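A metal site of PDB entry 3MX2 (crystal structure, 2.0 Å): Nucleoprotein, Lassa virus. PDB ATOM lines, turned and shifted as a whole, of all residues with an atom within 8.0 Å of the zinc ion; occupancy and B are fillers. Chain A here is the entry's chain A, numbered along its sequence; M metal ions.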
ATOM      1  N   GLU A 399     -19.060 -26.811   3.045  1.00  0.00           N
ATOM      2  CA  GLU A 399     -17.765 -27.414   3.038  1.00  0.00           C
ATOM      3  C   GLU A 399     -17.308 -27.460   4.481  1.00  0.00           C
ATOM      4  O   GLU A 399     -17.618 -26.558   5.287  1.00  0.00           O
ATOM      5  CB  GLU A 399     -16.813 -26.613   2.160  1.00  0.00           C
ATOM      6  CG  GLU A 399     -17.002 -26.888   0.699  1.00  0.00           C
ATOM      7  CD  GLU A 399     -16.656 -28.323   0.340  1.00  0.00           C
ATOM      8  OE1 GLU A 399     -15.665 -28.875   0.885  1.00  0.00           O
ATOM      9  OE2 GLU A 399     -17.386 -28.896  -0.485  1.00  0.00           O
ATOM     10  N   GLU A 407     -17.670 -23.178   5.115  1.00  0.00           N
ATOM     11  CA  GLU A 407     -18.327 -22.471   3.993  1.00  0.00           C
ATOM     12  C   GLU A 407     -19.742 -23.001   3.894  1.00  0.00           C
ATOM     13  O   GLU A 407     -19.951 -24.211   3.812  1.00  0.00           O
ATOM     14  CB  GLU A 407     -17.566 -22.624   2.640  1.00  0.00           C
ATOM     15  CG  GLU A 407     -18.005 -21.629   1.491  1.00  0.00           C
ATOM     16  CD  GLU A 407     -17.416 -21.959   0.094  1.00  0.00           C
ATOM     17  OE1 GLU A 407     -17.135 -23.167  -0.143  1.00  0.00           O
ATOM     18  OE2 GLU A 407     -17.230 -21.032  -0.779  1.00  0.00           O
ATOM     19  N   ILE A 408     -20.693 -22.089   3.943  1.00  0.00           N
ATOM     20  CA  ILE A 408     -22.104 -22.435   3.878  1.00  0.00           C
ATOM     21  C   ILE A 408     -22.692 -21.674   2.689  1.00  0.00           C
ATOM     22  O   ILE A 408     -22.356 -20.515   2.475  1.00  0.00           O
ATOM     23  CB  ILE A 408     -22.849 -21.986   5.167  1.00  0.00           C
ATOM     24  CG1 ILE A 408     -22.107 -22.399   6.452  1.00  0.00           C
ATOM     25  CG2 ILE A 408     -24.323 -22.386   5.148  1.00  0.00           C
ATOM     26  CD1 ILE A 408     -22.478 -23.710   7.036  1.00  0.00           C
ATOM     27  N   ALA A 409     -23.571 -22.335   1.930  1.00  0.00           N
ATOM     28  CA  ALA A 409     -24.339 -21.688   0.848  1.00  0.00           C
ATOM     29  C   ALA A 409     -25.761 -22.239   0.699  1.00  0.00           C
ATOM     30  O   ALA A 409     -25.986 -23.437   0.895  1.00  0.00           O
ATOM     31  CB  ALA A 409     -23.585 -21.804  -0.461  1.00  0.00           C
ATOM     32  N   HIS A 420     -24.210 -16.888   0.903  1.00  0.00           N
ATOM     33  CA  HIS A 420     -22.830 -17.380   0.880  1.00  0.00           C
ATOM     34  C   HIS A 420     -21.966 -16.696   1.927  1.00  0.00           C
ATOM     35  O   HIS A 420     -21.820 -15.449   1.930  1.00  0.00           O
ATOM     36  CB  HIS A 420     -22.226 -17.210  -0.506  1.00  0.00           C
ATOM     37  CG  HIS A 420     -20.865 -17.800  -0.670  1.00  0.00           C
ATOM     38  ND1 HIS A 420     -19.892 -17.198  -1.437  1.00  0.00           N
ATOM     39  CD2 HIS A 420     -20.319 -18.940  -0.190  1.00  0.00           C
ATOM     40  CE1 HIS A 420     -18.809 -17.952  -1.436  1.00  0.00           C
ATOM     41  NE2 HIS A 420     -19.042 -19.017  -0.679  1.00  0.00           N
ATOM     42  N   PHE A 421     -21.363 -17.513   2.792  1.00  0.00           N
ATOM     43  CA  PHE A 421     -20.482 -17.020   3.849  1.00  0.00           C
ATOM     44  C   PHE A 421     -19.529 -18.095   4.391  1.00  0.00           C
ATOM     45  O   PHE A 421     -19.576 -19.239   3.956  1.00  0.00           O
ATOM     46  CB  PHE A 421     -21.313 -16.392   4.986  1.00  0.00           C
ATOM     47  CG  PHE A 421     -22.274 -17.350   5.639  1.00  0.00           C
ATOM     48  CD1 PHE A 421     -22.014 -17.855   6.913  1.00  0.00           C
ATOM     49  CD2 PHE A 421     -23.431 -17.770   4.982  1.00  0.00           C
ATOM     50  CE1 PHE A 421     -22.898 -18.745   7.523  1.00  0.00           C
ATOM     51  CE2 PHE A 421     -24.336 -18.650   5.585  1.00  0.00           C
ATOM     52  CZ  PHE A 421     -24.053 -19.162   6.852  1.00  0.00           C
ATOM     53  N   PHE A 422     -18.665 -17.710   5.327  1.00  0.00           N
ATOM     54  CA  PHE A 422     -17.578 -18.560   5.767  1.00  0.00           C
ATOM     55  C   PHE A 422     -17.541 -18.630   7.294  1.00  0.00           C
ATOM     56  O   PHE A 422     -18.308 -17.929   7.973  1.00  0.00           O
ATOM     57  CB  PHE A 422     -16.251 -18.036   5.198  1.00  0.00           C
ATOM     58  CG  PHE A 422     -16.271 -17.875   3.708  1.00  0.00           C
ATOM     59  CD1 PHE A 422     -15.994 -18.961   2.872  1.00  0.00           C
ATOM     60  CD2 PHE A 422     -16.592 -16.660   3.133  1.00  0.00           C
ATOM     61  CE1 PHE A 422     -16.034 -18.811   1.479  1.00  0.00           C
ATOM     62  CE2 PHE A 422     -16.633 -16.483   1.753  1.00  0.00           C
ATOM     63  CZ  PHE A 422     -16.361 -17.565   0.924  1.00  0.00           C
ATOM     64  N   HIS A 439     -11.707 -28.614  -0.377  1.00  0.00           N
ATOM     65  CA  HIS A 439     -11.981 -27.197  -0.626  1.00  0.00           C
ATOM     66  C   HIS A 439     -10.816 -26.268  -0.963  1.00  0.00           C
ATOM     67  O   HIS A 439     -11.042 -25.216  -1.549  1.00  0.00           O
ATOM     68  CB  HIS A 439     -12.860 -26.582   0.481  1.00  0.00           C
ATOM     69  CG  HIS A 439     -12.316 -26.735   1.866  1.00  0.00           C
ATOM     70  ND1 HIS A 439     -11.091 -26.228   2.237  1.00  0.00           N
ATOM     71  CD2 HIS A 439     -12.826 -27.312   2.983  1.00  0.00           C
ATOM     72  CE1 HIS A 439     -10.871 -26.488   3.509  1.00  0.00           C
ATOM     73  NE2 HIS A 439     -11.908 -27.148   3.986  1.00  0.00           N
ATOM     74  N   ILE A 441      -9.186 -24.328   0.766  1.00  0.00           N
ATOM     75  CA  ILE A 441      -9.160 -23.069   1.465  1.00  0.00           C
ATOM     76  C   ILE A 441      -7.951 -22.973   2.399  1.00  0.00           C
ATOM     77  O   ILE A 441      -7.670 -23.907   3.171  1.00  0.00           O
ATOM     78  CB  ILE A 441     -10.475 -22.806   2.239  1.00  0.00           C
ATOM     79  CG1 ILE A 441     -11.688 -23.045   1.331  1.00  0.00           C
ATOM     80  CG2 ILE A 441     -10.470 -21.364   2.699  1.00  0.00           C
ATOM     81  CD1 ILE A 441     -13.046 -23.148   2.062  1.00  0.00           C
ATOM     82  N   TRP A 507     -18.293 -23.024 -13.112  1.00  0.00           N
ATOM     83  CA  TRP A 507     -17.137 -22.177 -12.797  1.00  0.00           C
ATOM     84  C   TRP A 507     -16.866 -21.145 -13.885  1.00  0.00           C
ATOM     85  O   TRP A 507     -16.521 -20.008 -13.584  1.00  0.00           O
ATOM     86  CB  TRP A 507     -15.905 -23.051 -12.572  1.00  0.00           C
ATOM     87  CG  TRP A 507     -15.836 -23.688 -11.189  1.00  0.00           C
ATOM     88  CD1 TRP A 507     -16.033 -25.019 -10.881  1.00  0.00           C
ATOM     89  CD2 TRP A 507     -15.535 -23.030  -9.951  1.00  0.00           C
ATOM     90  NE1 TRP A 507     -15.887 -25.212  -9.522  1.00  0.00           N
ATOM     91  CE2 TRP A 507     -15.578 -24.015  -8.929  1.00  0.00           C
ATOM     92  CE3 TRP A 507     -15.220 -21.692  -9.609  1.00  0.00           C
ATOM     93  CZ2 TRP A 507     -15.310 -23.711  -7.583  1.00  0.00           C
ATOM     94  CZ3 TRP A 507     -15.001 -21.396  -8.257  1.00  0.00           C
ATOM     95  CH2 TRP A 507     -15.042 -22.405  -7.262  1.00  0.00           C
ATOM     96  N   LYS A 511     -17.208 -17.796 -11.655  1.00  0.00           N
ATOM     97  CA  LYS A 511     -15.940 -17.738 -10.927  1.00  0.00           C
ATOM     98  C   LYS A 511     -15.794 -16.508 -10.002  1.00  0.00           C
ATOM     99  O   LYS A 511     -15.289 -16.628  -8.891  1.00  0.00           O
ATOM    100  CB  LYS A 511     -14.701 -17.852 -11.844  1.00  0.00           C
ATOM    101  CG  LYS A 511     -13.343 -17.511 -11.159  1.00  0.00           C
ATOM    102  CD  LYS A 511     -12.940 -18.620 -10.142  1.00  0.00           C
ATOM    103  CE  LYS A 511     -11.817 -18.131  -9.182  1.00  0.00           C
ATOM    104  NZ  LYS A 511     -12.282 -16.945  -8.388  1.00  0.00           N
ATOM    105  N   LEU A 513     -17.728 -15.016  -8.290  1.00  0.00           N
ATOM    106  CA  LEU A 513     -18.528 -15.051  -7.063  1.00  0.00           C
ATOM    107  C   LEU A 513     -17.876 -15.706  -5.851  1.00  0.00           C
ATOM    108  O   LEU A 513     -18.401 -15.583  -4.761  1.00  0.00           O
ATOM    109  CB  LEU A 513     -19.893 -15.671  -7.323  1.00  0.00           C
ATOM    110  CG  LEU A 513     -20.720 -14.935  -8.385  1.00  0.00           C
ATOM    111  CD1 LEU A 513     -21.963 -15.733  -8.655  1.00  0.00           C
ATOM    112  CD2 LEU A 513     -21.038 -13.484  -8.025  1.00  0.00           C
ATOM    113  N   CYS A 514     -16.786 -16.453  -6.022  1.00  0.00           N
ATOM    114  CA  CYS A 514     -16.030 -16.945  -4.863  1.00  0.00           C
ATOM    115  C   CYS A 514     -14.548 -17.001  -5.142  1.00  0.00           C
ATOM    116  O   CYS A 514     -14.127 -17.685  -6.091  1.00  0.00           O
ATOM    117  CB  CYS A 514     -16.522 -18.322  -4.366  1.00  0.00           C
ATOM    118  SG  CYS A 514     -15.661 -18.752  -2.795  1.00  0.00           S
ATOM    119  N   HIS A 515     -13.773 -16.321  -4.281  1.00  0.00           N
ATOM    120  CA  HIS A 515     -12.333 -16.207  -4.432  1.00  0.00           C
ATOM    121  C   HIS A 515     -11.567 -17.001  -3.361  1.00  0.00           C
ATOM    122  O   HIS A 515     -10.361 -16.794  -3.168  1.00  0.00           O
ATOM    123  CB  HIS A 515     -11.923 -14.716  -4.388  1.00  0.00           C
ATOM    124  CG  HIS A 515     -12.555 -13.882  -5.471  1.00  0.00           C
ATOM    125  ND1 HIS A 515     -11.934 -13.666  -6.692  1.00  0.00           N
ATOM    126  CD2 HIS A 515     -13.731 -13.209  -5.515  1.00  0.00           C
ATOM    127  CE1 HIS A 515     -12.705 -12.902  -7.443  1.00  0.00           C
ATOM    128  NE2 HIS A 515     -13.806 -12.613  -6.762  1.00  0.00           N
ATOM    129  N   MET A 516     -12.254 -17.919  -2.682  1.00  0.00           N
ATOM    130  CA  MET A 516     -11.741 -18.493  -1.438  1.00  0.00           C
ATOM    131  C   MET A 516     -10.915 -19.771  -1.620  1.00  0.00           C
ATOM    132  O   MET A 516     -10.067 -20.101  -0.779  1.00  0.00           O
ATOM    133  CB  MET A 516     -12.886 -18.616  -0.403  1.00  0.00           C
ATOM    134  CG  MET A 516     -12.510 -18.981   1.025  1.00  0.00           C
ATOM    135  SD  MET A 516     -11.446 -17.733   1.841  1.00  0.00           S
ATOM    136  CE  MET A 516     -12.723 -16.569   2.288  1.00  0.00           C
ATOM    137  N   HIS A 517     -11.110 -20.450  -2.741  1.00  0.00           N
ATOM    138  CA  HIS A 517     -10.445 -21.702  -3.016  1.00  0.00           C
ATOM    139  C   HIS A 517      -9.122 -21.472  -3.782  1.00  0.00           C
ATOM    140  O   HIS A 517      -9.112 -21.170  -4.982  1.00  0.00           O
ATOM    141  CB  HIS A 517     -11.450 -22.669  -3.683  1.00  0.00           C
ATOM    142  CG  HIS A 517     -12.784 -22.699  -2.969  1.00  0.00           C
ATOM    143  ND1 HIS A 517     -13.112 -23.659  -2.040  1.00  0.00           N
ATOM    144  CD2 HIS A 517     -13.835 -21.840  -3.023  1.00  0.00           C
ATOM    145  CE1 HIS A 517     -14.326 -23.403  -1.562  1.00  0.00           C
ATOM    146  NE2 HIS A 517     -14.785 -22.308  -2.144  1.00  0.00           N
ATOM    147  N   PRO A 535     -11.218 -27.571  -6.949  1.00  0.00           N
ATOM    148  CA  PRO A 535     -11.745 -27.504  -5.566  1.00  0.00           C
ATOM    149  C   PRO A 535     -13.269 -27.420  -5.454  1.00  0.00           C
ATOM    150  O   PRO A 535     -13.940 -26.896  -6.362  1.00  0.00           O
ATOM    151  CB  PRO A 535     -11.136 -26.238  -4.980  1.00  0.00           C
ATOM    152  CG  PRO A 535     -10.001 -25.863  -5.917  1.00  0.00           C
ATOM    153  CD  PRO A 535     -10.263 -26.483  -7.252  1.00  0.00           C
ATOM    154  N   HIS A 536     -13.797 -27.890  -4.322  1.00  0.00           N
ATOM    155  CA  HIS A 536     -15.224 -27.917  -4.070  1.00  0.00           C
ATOM    156  C   HIS A 536     -15.610 -26.650  -3.322  1.00  0.00           C
ATOM    157  O   HIS A 536     -15.028 -26.359  -2.272  1.00  0.00           O
ATOM    158  CB  HIS A 536     -15.609 -29.126  -3.210  1.00  0.00           C
ATOM    159  CG  HIS A 536     -15.339 -30.455  -3.853  1.00  0.00           C
ATOM    160  ND1 HIS A 536     -15.270 -30.634  -5.219  1.00  0.00           N
ATOM    161  CD2 HIS A 536     -15.167 -31.680  -3.304  1.00  0.00           C
ATOM    162  CE1 HIS A 536     -15.031 -31.908  -5.483  1.00  0.00           C
ATOM    163  NE2 HIS A 536     -14.968 -32.563  -4.338  1.00  0.00           N
ATOM    164  N   CYS A 537     -16.547 -25.889  -3.888  1.00  0.00           N
ATOM    165  CA  CYS A 537     -17.084 -24.681  -3.281  1.00  0.00           C
ATOM    166  C   CYS A 537     -18.554 -24.939  -2.976  1.00  0.00           C
ATOM    167  O   CYS A 537     -19.283 -25.402  -3.812  1.00  0.00           O
ATOM    168  CB  CYS A 537     -16.929 -23.499  -4.261  1.00  0.00           C
ATOM    169  SG  CYS A 537     -17.980 -22.056  -3.966  1.00  0.00           S
ATOM    170  N   ALA A 538     -18.978 -24.590  -1.759  1.00  0.00           N
ATOM    171  CA  ALA A 538     -20.367 -24.665  -1.360  1.00  0.00           C
ATOM    172  C   ALA A 538     -21.372 -24.003  -2.306  1.00  0.00           C
ATOM    173  O   ALA A 538     -22.408 -24.565  -2.587  1.00  0.00           O
ATOM    174  CB  ALA A 538     -20.536 -24.149   0.062  1.00  0.00           C
ATOM    175  N   LEU A 539     -21.048 -22.823  -2.808  1.00  0.00           N
ATOM    176  CA  LEU A 539     -21.930 -22.106  -3.727  1.00  0.00           C
ATOM    177  C   LEU A 539     -21.962 -22.790  -5.086  1.00  0.00           C
ATOM    178  O   LEU A 539     -23.037 -23.119  -5.604  1.00  0.00           O
ATOM    179  CB  LEU A 539     -21.523 -20.628  -3.854  1.00  0.00           C
ATOM    180  CG  LEU A 539     -22.371 -19.733  -4.781  1.00  0.00           C
ATOM    181  CD1 LEU A 539     -23.854 -19.766  -4.420  1.00  0.00           C
ATOM    182  CD2 LEU A 539     -21.861 -18.281  -4.763  1.00  0.00           C
ATOM    183  N   MET A 540     -20.789 -23.066  -5.639  1.00  0.00           N
ATOM    184  CA  MET A 540     -20.744 -23.710  -6.958  1.00  0.00           C
ATOM    185  C   MET A 540     -21.370 -25.096  -6.974  1.00  0.00           C
ATOM    186  O   MET A 540     -22.026 -25.437  -7.950  1.00  0.00           O
ATOM    187  CB  MET A 540     -19.350 -23.746  -7.541  1.00  0.00           C
ATOM    188  CG  MET A 540     -18.668 -22.361  -7.482  1.00  0.00           C
ATOM    189  SD  MET A 540     -19.413 -21.206  -8.645  1.00  0.00           S
ATOM    190  CE  MET A 540     -19.708 -19.812  -7.582  1.00  0.00           C
ATOM    191  N   ASP A 541     -21.173 -25.869  -5.913  1.00  0.00           N
ATOM    192  CA  ASP A 541     -21.878 -27.133  -5.766  1.00  0.00           C
ATOM    193  C   ASP A 541     -23.426 -26.995  -5.819  1.00  0.00           C
ATOM    194  O   ASP A 541     -24.061 -27.752  -6.550  1.00  0.00           O
ATOM    195  CB  ASP A 541     -21.419 -27.869  -4.499  1.00  0.00           C
ATOM    196  CG  ASP A 541     -20.051 -28.503  -4.649  1.00  0.00           C
ATOM    197  OD1 ASP A 541     -19.444 -28.478  -5.762  1.00  0.00           O
ATOM    198  OD2 ASP A 541     -19.560 -29.061  -3.645  1.00  0.00           O
HETATM  199 ZN    ZN M   1     -16.647 -20.842  -2.594  1.00  0.00          ZN
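NE2 of His 420 touches the zinc ion (3.6 Å). Within 4 Å of the zinc ion: Glu 407, His 420, Cys 514, His 517 and Cys 537. The nearest printed residue that does not touch the zinc ion is Ala 538 (4.5 Å).
The side-chain carboxylate (OE2) of Glu 407 is bound to the zinc ion (1.9 Å). SG of Cys 537 binds the zinc ion, at 2.3 Å. The side-chain sulfur (SG) of Cys 514 is bound to the zinc ion, 2.3 Å away. NE2 of His 517 binds the zinc ion (2.4 Å). The zinc ion has four donor atoms within binding distance.
OE2 of Glu 407 lies close to NE2 of His 420 (2.7 Å). The backbone carbonyl oxygen (O) of Glu 407 sits at hydrogen-bond distance from the backbone NH (N) of Glu 399 (2.9 Å). The side-chain sulfur of Cys 537 lies close to the backbone NH of Leu 539. The side-chain sulfur (SG) of Cys 537 sits close to the backbone NH (N) of Met 540 (3.4 Å). SG of Cys 514 lies close to N of Met 516 (3.5 Å). NZ of Lys 511 sits at hydrogen-bond distance from O of Cys 514, 3.0 Å away. A ring nitrogen (ND1) of His 517 lies close to the backbone carbonyl oxygen (O) of His 536 (3.3 Å). ND1 of His 517 lies within hydrogen-bond range of O of His 439, at 2.6 Å.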
